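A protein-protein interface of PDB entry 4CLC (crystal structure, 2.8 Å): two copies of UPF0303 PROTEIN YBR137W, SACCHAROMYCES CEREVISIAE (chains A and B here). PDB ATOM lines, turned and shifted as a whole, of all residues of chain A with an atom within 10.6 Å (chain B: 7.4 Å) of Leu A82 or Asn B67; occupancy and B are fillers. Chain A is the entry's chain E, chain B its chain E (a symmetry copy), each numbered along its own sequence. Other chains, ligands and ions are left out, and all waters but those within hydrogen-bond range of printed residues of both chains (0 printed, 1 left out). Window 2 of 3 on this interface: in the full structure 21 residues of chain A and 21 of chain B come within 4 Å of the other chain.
No position is printed for both chains.
Of the 10 pairs that touch across the chains among the printed residues, none has its exchanged pair printed and touching as well.
Of the printed residues of chain B, Val A75 touches His B69.
Gly A78 touches none of the printed residues of chain B.
Printed residues of chain B within 4 Å of Ser A80: His B69.
Leu A82 touches three residues of chain B.
Printed residues of chain B within 4 Å of Asp A85: Gly B68, His B69 and Cys B70.
Asn B67 touches just one residue of chain A: Leu A82.
Of chain A, only Leu A82 and Asp A85 come within 4 Å of Gly B68.
Printed residues of chain A within 4 Å of His B69: Val A75, Ser A80, Ala A81, Leu A82 and Asp A85.
Of the printed residues of chain A, Cys B70 touches Arg A73 (3.7 Å) and Asp A85 (2.9 Å).
O of Ala A81 sits close to NE2 of His B69 (3.3 Å).
OD2 of Asp A85 is in hydrogen-bond range of N of Cys B70.
The guanidinium group (NH1) of Arg A73 lies within salt-bridge range of the side-chain carboxylate (OD1) of Asp A85 (3.9 Å).
The backbone NH of Ala A81 lies close to the side-chain amide nitrogen of Asn A84 (3.2 Å).
The side-chain amide oxygen of Asn B67 lies within hydrogen-bond range of the backbone NH of His B69, at 3.3 Å.
Printed residues of chain B that touch a printed residue of chain A: Asn B67, Gly B68, His B69 and Cys B70.
Hydrophobic or aromatic side chains of chain B within 4 Å of the printed part of chain A: His B69.
Printed residues of chain A that touch a printed residue of chain B: Arg A73, Val A75, Ser A80, Ala A81, Leu A82 and Asp A85.
Hydrophobic or aromatic side chains of chain A within 4 Å of the printed part of chain B: Val A75 and Leu A82.
Among the printed residues, no Asp or Glu carboxylate lies within 4 Å of a Lys or Arg side-chain nitrogen of the other chain.
Arg A73 touches Cys B70.
CG1 of Val A75 touches NE2 of His B69 (3.9 Å).
OG of Ser A80 touches CE1 of His B69, at 3.3 Å.
CB of Leu A82 touches ND2 of Asn B67, 3.6 Å away.
Gly B68 touches Leu A82 (C to CD1, 3.8 Å).
Leu A82 touches His B69 (CD1 to N, 3.6 Å).
O of Gly B68 touches OD2 of Asp A85 (3.8 Å).
OD1 of Asp A85 touches CD2 of His B69 (2.9 Å).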
ATOM      1  N   PRO A  58     -32.733  14.117  37.050  1.00  0.00           N
ATOM      2  CA  PRO A  58     -32.052  14.449  35.793  1.00  0.00           C
ATOM      3  C   PRO A  58     -30.809  13.570  35.534  1.00  0.00           C
ATOM      4  O   PRO A  58     -29.694  13.867  35.973  1.00  0.00           O
ATOM      5  CB  PRO A  58     -31.682  15.924  35.983  1.00  0.00           C
ATOM      6  CG  PRO A  58     -31.554  16.104  37.438  1.00  0.00           C
ATOM      7  CD  PRO A  58     -32.499  15.140  38.086  1.00  0.00           C
ATOM      8  N   ALA A  60     -28.199  11.471  32.860  1.00  0.00           N
ATOM      9  CA  ALA A  60     -27.680  11.319  31.481  1.00  0.00           C
ATOM     10  C   ALA A  60     -27.217   9.893  31.189  1.00  0.00           C
ATOM     11  O   ALA A  60     -26.500   9.280  31.993  1.00  0.00           O
ATOM     12  CB  ALA A  60     -26.548  12.280  31.221  1.00  0.00           C
ATOM     13  N   ARG A  73     -27.148   8.810  23.285  1.00  0.00           N
ATOM     14  CA  ARG A  73     -27.117   9.745  24.398  1.00  0.00           C
ATOM     15  C   ARG A  73     -28.519  10.235  24.704  1.00  0.00           C
ATOM     16  O   ARG A  73     -29.255  10.596  23.785  1.00  0.00           O
ATOM     17  CB  ARG A  73     -26.222  10.933  24.081  1.00  0.00           C
ATOM     18  CG  ARG A  73     -26.254  11.996  25.137  1.00  0.00           C
ATOM     19  CD  ARG A  73     -25.462  11.540  26.322  1.00  0.00           C
ATOM     20  NE  ARG A  73     -24.135  11.093  25.919  1.00  0.00           N
ATOM     21  CZ  ARG A  73     -23.039  11.831  25.993  1.00  0.00           C
ATOM     22  NH1 ARG A  73     -23.087  13.079  26.462  1.00  0.00           N
ATOM     23  NH2 ARG A  73     -21.890  11.308  25.601  1.00  0.00           N
ATOM     24  N   VAL A  75     -30.944  12.445  28.060  1.00  0.00           N
ATOM     25  CA  VAL A  75     -31.211  12.921  29.409  1.00  0.00           C
ATOM     26  C   VAL A  75     -32.642  12.552  29.778  1.00  0.00           C
ATOM     27  O   VAL A  75     -33.528  12.529  28.923  1.00  0.00           O
ATOM     28  CB  VAL A  75     -30.979  14.444  29.538  1.00  0.00           C
ATOM     29  CG1 VAL A  75     -29.502  14.742  29.388  1.00  0.00           C
ATOM     30  CG2 VAL A  75     -31.793  15.202  28.510  1.00  0.00           C
ATOM     31  N   GLY A  78     -35.631  17.112  33.396  1.00  0.00           N
ATOM     32  CA  GLY A  78     -35.250  18.442  32.975  1.00  0.00           C
ATOM     33  C   GLY A  78     -34.062  19.150  33.612  1.00  0.00           C
ATOM     34  O   GLY A  78     -33.709  20.252  33.178  1.00  0.00           O
ATOM     35  N   GLY A  79     -33.425  18.576  34.621  1.00  0.00           N
ATOM     36  CA  GLY A  79     -32.339  19.308  35.266  1.00  0.00           C
ATOM     37  C   GLY A  79     -30.890  18.993  34.893  1.00  0.00           C
ATOM     38  O   GLY A  79     -29.986  19.222  35.701  1.00  0.00           O
ATOM     39  N   SER A  80     -30.661  18.431  33.704  1.00  0.00           N
ATOM     40  CA  SER A  80     -29.311  18.030  33.284  1.00  0.00           C
ATOM     41  C   SER A  80     -28.503  19.226  32.822  1.00  0.00           C
ATOM     42  O   SER A  80     -29.058  20.263  32.489  1.00  0.00           O
ATOM     43  CB  SER A  80     -29.365  16.974  32.182  1.00  0.00           C
ATOM     44  OG  SER A  80     -30.316  17.303  31.184  1.00  0.00           O
ATOM     45  N   ALA A  81     -27.186  19.092  32.826  1.00  0.00           N
ATOM     46  CA  ALA A  81     -26.330  20.208  32.456  1.00  0.00           C
ATOM     47  C   ALA A  81     -25.045  19.713  31.805  1.00  0.00           C
ATOM     48  O   ALA A  81     -24.798  18.505  31.735  1.00  0.00           O
ATOM     49  CB  ALA A  81     -26.016  21.047  33.665  1.00  0.00           C
ATOM     50  N   LEU A  82     -24.211  20.648  31.357  1.00  0.00           N
ATOM     51  CA  LEU A  82     -23.005  20.275  30.638  1.00  0.00           C
ATOM     52  C   LEU A  82     -22.100  19.424  31.526  1.00  0.00           C
ATOM     53  O   LEU A  82     -21.260  18.658  31.037  1.00  0.00           O
ATOM     54  CB  LEU A  82     -22.257  21.519  30.138  1.00  0.00           C
ATOM     55  CG  LEU A  82     -20.981  21.231  29.327  1.00  0.00           C
ATOM     56  CD1 LEU A  82     -21.317  20.572  28.007  1.00  0.00           C
ATOM     57  CD2 LEU A  82     -20.162  22.464  29.129  1.00  0.00           C
ATOM     58  N   ASP A  83     -22.280  19.549  32.835  1.00  0.00           N
ATOM     59  CA  ASP A  83     -21.418  18.842  33.772  1.00  0.00           C
ATOM     60  C   ASP A  83     -21.636  17.342  33.686  1.00  0.00           C
ATOM     61  O   ASP A  83     -20.708  16.564  33.886  1.00  0.00           O
ATOM     62  CB  ASP A  83     -21.648  19.332  35.200  1.00  0.00           C
ATOM     63  CG  ASP A  83     -20.657  18.743  36.171  1.00  0.00           C
ATOM     64  OD1 ASP A  83     -19.450  19.039  36.010  1.00  0.00           O
ATOM     65  OD2 ASP A  83     -21.076  18.007  37.092  1.00  0.00           O
ATOM     66  N   ASN A  84     -22.869  16.952  33.384  1.00  0.00           N
ATOM     67  CA  ASN A  84     -23.170  15.563  33.116  1.00  0.00           C
ATOM     68  C   ASN A  84     -22.318  14.995  31.991  1.00  0.00           C
ATOM     69  O   ASN A  84     -21.845  13.871  32.086  1.00  0.00           O
ATOM     70  CB  ASN A  84     -24.640  15.400  32.766  1.00  0.00           C
ATOM     71  CG  ASN A  84     -25.533  15.452  33.983  1.00  0.00           C
ATOM     72  OD1 ASN A  84     -25.212  14.878  35.041  1.00  0.00           O
ATOM     73  ND2 ASN A  84     -26.673  16.142  33.847  1.00  0.00           N
ATOM     74  N   ASP A  85     -22.139  15.786  30.934  1.00  0.00           N
ATOM     75  CA  ASP A  85     -21.365  15.419  29.759  1.00  0.00           C
ATOM     76  C   ASP A  85     -19.919  15.148  30.137  1.00  0.00           C
ATOM     77  O   ASP A  85     -19.278  14.226  29.622  1.00  0.00           O
ATOM     78  CB  ASP A  85     -21.424  16.536  28.717  1.00  0.00           C
ATOM     79  CG  ASP A  85     -22.772  16.638  28.017  1.00  0.00           C
ATOM     80  OD1 ASP A  85     -23.798  16.267  28.615  1.00  0.00           O
ATOM     81  OD2 ASP A  85     -22.799  17.098  26.858  1.00  0.00           O
ATOM     82  N   PHE A  86     -19.405  15.975  31.040  1.00  0.00           N
ATOM     83  CA  PHE A  86     -18.066  15.778  31.579  1.00  0.00           C
ATOM     84  C   PHE A  86     -17.967  14.506  32.411  1.00  0.00           C
ATOM     85  O   PHE A  86     -16.977  13.804  32.335  1.00  0.00           O
ATOM     86  CB  PHE A  86     -17.644  16.972  32.429  1.00  0.00           C
ATOM     87  CG  PHE A  86     -17.145  18.130  31.639  1.00  0.00           C
ATOM     88  CD1 PHE A  86     -18.019  19.097  31.169  1.00  0.00           C
ATOM     89  CD2 PHE A  86     -15.795  18.266  31.361  1.00  0.00           C
ATOM     90  CE1 PHE A  86     -17.545  20.156  30.439  1.00  0.00           C
ATOM     91  CE2 PHE A  86     -15.333  19.329  30.639  1.00  0.00           C
ATOM     92  CZ  PHE A  86     -16.195  20.268  30.187  1.00  0.00           C
ATOM     93  N   TRP A  87     -18.985  14.229  33.221  1.00  0.00           N
ATOM     94  CA  TRP A  87     -18.966  13.046  34.067  1.00  0.00           C
ATOM     95  C   TRP A  87     -18.970  11.803  33.212  1.00  0.00           C
ATOM     96  O   TRP A  87     -18.200  10.874  33.481  1.00  0.00           O
ATOM     97  CB  TRP A  87     -20.144  13.018  35.044  1.00  0.00           C
ATOM     98  CG  TRP A  87     -19.849  13.764  36.309  1.00  0.00           C
ATOM     99  CD1 TRP A  87     -20.312  14.995  36.665  1.00  0.00           C
ATOM    100  CD2 TRP A  87     -18.998  13.326  37.381  1.00  0.00           C
ATOM    101  NE1 TRP A  87     -19.806  15.350  37.892  1.00  0.00           N
ATOM    102  CE2 TRP A  87     -19.010  14.357  38.347  1.00  0.00           C
ATOM    103  CE3 TRP A  87     -18.242  12.179  37.603  1.00  0.00           C
ATOM    104  CZ2 TRP A  87     -18.276  14.255  39.526  1.00  0.00           C
ATOM    105  CZ3 TRP A  87     -17.519  12.090  38.773  1.00  0.00           C
ATOM    106  CH2 TRP A  87     -17.543  13.130  39.725  1.00  0.00           C
ATOM    107  N   ILE A  88     -19.818  11.802  32.181  1.00  0.00           N
ATOM    108  CA  ILE A  88     -19.877  10.705  31.223  1.00  0.00           C
ATOM    109  C   ILE A  88     -18.533  10.500  30.547  1.00  0.00           C
ATOM    110  O   ILE A  88     -18.049   9.376  30.475  1.00  0.00           O
ATOM    111  CB  ILE A  88     -20.941  10.944  30.161  1.00  0.00           C
ATOM    112  CG1 ILE A  88     -22.316  10.831  30.783  1.00  0.00           C
ATOM    113  CG2 ILE A  88     -20.837   9.925  29.052  1.00  0.00           C
ATOM    114  CD1 ILE A  88     -23.382  11.260  29.853  1.00  0.00           C
ATOM    115  N   GLN A  89     -17.916  11.586  30.079  1.00  0.00           N
ATOM    116  CA  GLN A  89     -16.578  11.482  29.499  1.00  0.00           C
ATOM    117  C   GLN A  89     -15.659  10.845  30.495  1.00  0.00           C
ATOM    118  O   GLN A  89     -15.103   9.793  30.236  1.00  0.00           O
ATOM    119  CB  GLN A  89     -16.006  12.844  29.087  1.00  0.00           C
ATOM    120  CG  GLN A  89     -16.511  13.356  27.751  1.00  0.00           C
ATOM    121  CD  GLN A  89     -16.580  12.260  26.682  1.00  0.00           C
ATOM    122  OE1 GLN A  89     -17.647  11.661  26.445  1.00  0.00           O
ATOM    123  NE2 GLN A  89     -15.445  12.006  26.018  1.00  0.00           N
ATOM    124  N   ARG A  90     -15.536  11.466  31.658  1.00  0.00           N
ATOM    125  CA  ARG A  90     -14.564  11.031  32.651  1.00  0.00           C
ATOM    126  C   ARG A  90     -14.806   9.589  33.136  1.00  0.00           C
ATOM    127  O   ARG A  90     -13.859   8.819  33.342  1.00  0.00           O
ATOM    128  CB  ARG A  90     -14.572  12.007  33.821  1.00  0.00           C
ATOM    129  CG  ARG A  90     -14.179  13.397  33.416  1.00  0.00           C
ATOM    130  CD  ARG A  90     -14.332  14.412  34.516  1.00  0.00           C
ATOM    131  NE  ARG A  90     -13.486  14.093  35.660  1.00  0.00           N
ATOM    132  CZ  ARG A  90     -13.951  13.647  36.821  1.00  0.00           C
ATOM    133  NH1 ARG A  90     -15.256  13.480  37.002  1.00  0.00           N
ATOM    134  NH2 ARG A  90     -13.106  13.378  37.803  1.00  0.00           N
ATOM    135  N   SER A 149     -25.001   8.946  34.513  1.00  0.00           N
ATOM    136  CA  SER A 149     -24.577   9.955  35.481  1.00  0.00           C
ATOM    137  C   SER A 149     -25.748  10.757  36.028  1.00  0.00           C
ATOM    138  O   SER A 149     -26.718  11.032  35.315  1.00  0.00           O
ATOM    139  CB  SER A 149     -23.548  10.906  34.868  1.00  0.00           C
ATOM    140  OG  SER A 149     -23.329  12.027  35.707  1.00  0.00           O
ATOM    141  N   SER B  64     -28.255  19.440  20.655  1.00  0.00           N
ATOM    142  CA  SER B  64     -27.402  19.951  21.716  1.00  0.00           C
ATOM    143  C   SER B  64     -27.711  21.400  22.033  1.00  0.00           C
ATOM    144  O   SER B  64     -28.178  22.128  21.178  1.00  0.00           O
ATOM    145  CB  SER B  64     -25.935  19.810  21.327  1.00  0.00           C
ATOM    146  OG  SER B  64     -25.594  18.456  21.111  1.00  0.00           O
ATOM    147  N   LEU B  65     -27.437  21.817  23.261  1.00  0.00           N
ATOM    148  CA  LEU B  65     -27.662  23.197  23.680  1.00  0.00           C
ATOM    149  C   LEU B  65     -26.590  24.081  23.079  1.00  0.00           C
ATOM    150  O   LEU B  65     -25.620  23.577  22.551  1.00  0.00           O
ATOM    151  CB  LEU B  65     -27.664  23.310  25.209  1.00  0.00           C
ATOM    152  CG  LEU B  65     -28.800  22.565  25.912  1.00  0.00           C
ATOM    153  CD1 LEU B  65     -28.904  23.014  27.342  1.00  0.00           C
ATOM    154  CD2 LEU B  65     -30.137  22.736  25.181  1.00  0.00           C
ATOM    155  N   PRO B  66     -26.771  25.406  23.128  1.00  0.00           N
ATOM    156  CA  PRO B  66     -25.719  26.266  22.572  1.00  0.00           C
ATOM    157  C   PRO B  66     -24.422  26.232  23.361  1.00  0.00           C
ATOM    158  O   PRO B  66     -23.400  26.616  22.830  1.00  0.00           O
ATOM    159  CB  PRO B  66     -26.350  27.663  22.609  1.00  0.00           C
ATOM    160  CG  PRO B  66     -27.571  27.534  23.399  1.00  0.00           C
ATOM    161  CD  PRO B  66     -28.029  26.143  23.303  1.00  0.00           C
ATOM    162  N   ASN B  67     -24.468  25.782  24.604  1.00  0.00           N
ATOM    163  CA  ASN B  67     -23.280  25.632  25.419  1.00  0.00           C
ATOM    164  C   ASN B  67     -22.669  24.214  25.288  1.00  0.00           C
ATOM    165  O   ASN B  67     -21.720  23.849  25.984  1.00  0.00           O
ATOM    166  CB  ASN B  67     -23.619  25.924  26.866  1.00  0.00           C
ATOM    167  CG  ASN B  67     -24.244  24.724  27.572  1.00  0.00           C
ATOM    168  OD1 ASN B  67     -25.042  23.973  26.990  1.00  0.00           O
ATOM    169  ND2 ASN B  67     -23.859  24.523  28.832  1.00  0.00           N
ATOM    170  N   GLY B  68     -23.243  23.412  24.403  1.00  0.00           N
ATOM    171  CA  GLY B  68     -22.614  22.174  24.017  1.00  0.00           C
ATOM    172  C   GLY B  68     -23.203  20.948  24.679  1.00  0.00           C
ATOM    173  O   GLY B  68     -22.924  19.821  24.267  1.00  0.00           O
ATOM    174  N   HIS B  69     -24.015  21.159  25.707  1.00  0.00           N
ATOM    175  CA  HIS B  69     -24.615  20.054  26.430  1.00  0.00           C
ATOM    176  C   HIS B  69     -25.479  19.235  25.481  1.00  0.00           C
ATOM    177  O   HIS B  69     -26.350  19.769  24.825  1.00  0.00           O
ATOM    178  CB  HIS B  69     -25.443  20.571  27.604  1.00  0.00           C
ATOM    179  CG  HIS B  69     -26.204  19.499  28.319  1.00  0.00           C
ATOM    180  ND1 HIS B  69     -27.551  19.599  28.599  1.00  0.00           N
ATOM    181  CD2 HIS B  69     -25.808  18.293  28.794  1.00  0.00           C
ATOM    182  CE1 HIS B  69     -27.947  18.505  29.229  1.00  0.00           C
ATOM    183  NE2 HIS B  69     -26.911  17.696  29.355  1.00  0.00           N
ATOM    184  N   CYS B  70     -25.235  17.934  25.423  1.00  0.00           N
ATOM    185  CA  CYS B  70     -25.915  17.075  24.462  1.00  0.00           C
ATOM    186  C   CYS B  70     -27.174  16.425  25.041  1.00  0.00           C
ATOM    187  O   CYS B  70     -27.109  15.745  26.064  1.00  0.00           O
ATOM    188  CB  CYS B  70     -24.955  15.996  23.955  1.00  0.00           C
ATOM    189  SG  CYS B  70     -25.716  14.800  22.851  1.00  0.00           S
ATOM    190  N   LEU B  96     -23.801  27.510  15.474  1.00  0.00           N
ATOM    191  CA  LEU B  96     -23.923  28.277  16.706  1.00  0.00           C
ATOM    192  C   LEU B  96     -23.138  29.598  16.670  1.00  0.00           C
ATOM    193  O   LEU B  96     -23.659  30.635  17.092  1.00  0.00           O
ATOM    194  CB  LEU B  96     -23.501  27.422  17.888  1.00  0.00           C
ATOM    195  CG  LEU B  96     -24.373  26.188  18.119  1.00  0.00           C
ATOM    196  CD1 LEU B  96     -23.689  25.264  19.114  1.00  0.00           C
ATOM    197  CD2 LEU B  96     -25.755  26.574  18.612  1.00  0.00           C
ATOM    198  N   TYR B 143     -33.034  27.984  20.894  1.00  0.00           N
ATOM    199  CA  TYR B 143     -33.101  27.063  22.020  1.00  0.00           C
ATOM    200  C   TYR B 143     -31.868  26.187  22.036  1.00  0.00           C
ATOM    201  O   TYR B 143     -31.145  26.106  23.039  1.00  0.00           O
ATOM    202  CB  TYR B 143     -34.347  26.175  21.938  1.00  0.00           C
ATOM    203  CG  TYR B 143     -35.639  26.817  22.416  1.00  0.00           C
ATOM    204  CD1 TYR B 143     -35.655  27.698  23.477  1.00  0.00           C
ATOM    205  CD2 TYR B 143     -36.838  26.530  21.791  1.00  0.00           C
ATOM    206  CE1 TYR B 143     -36.828  28.265  23.898  1.00  0.00           C
ATOM    207  CE2 TYR B 143     -38.009  27.086  22.202  1.00  0.00           C
ATOM    208  CZ  TYR B 143     -38.009  27.953  23.253  1.00  0.00           C
ATOM    209  OH  TYR B 143     -39.210  28.516  23.660  1.00  0.00           O
ATOM    210  N   ALA B 144     -31.637  25.549  20.892  1.00  0.00           N
ATOM    211  CA  ALA B 144     -30.608  24.531  20.749  1.00  0.00           C
ATOM    212  C   ALA B 144     -30.314  24.290  19.272  1.00  0.00           C
ATOM    213  O   ALA B 144     -30.893  24.938  18.404  1.00  0.00           O
ATOM    214  CB  ALA B 144     -31.049  23.237  21.430  1.00  0.00           C
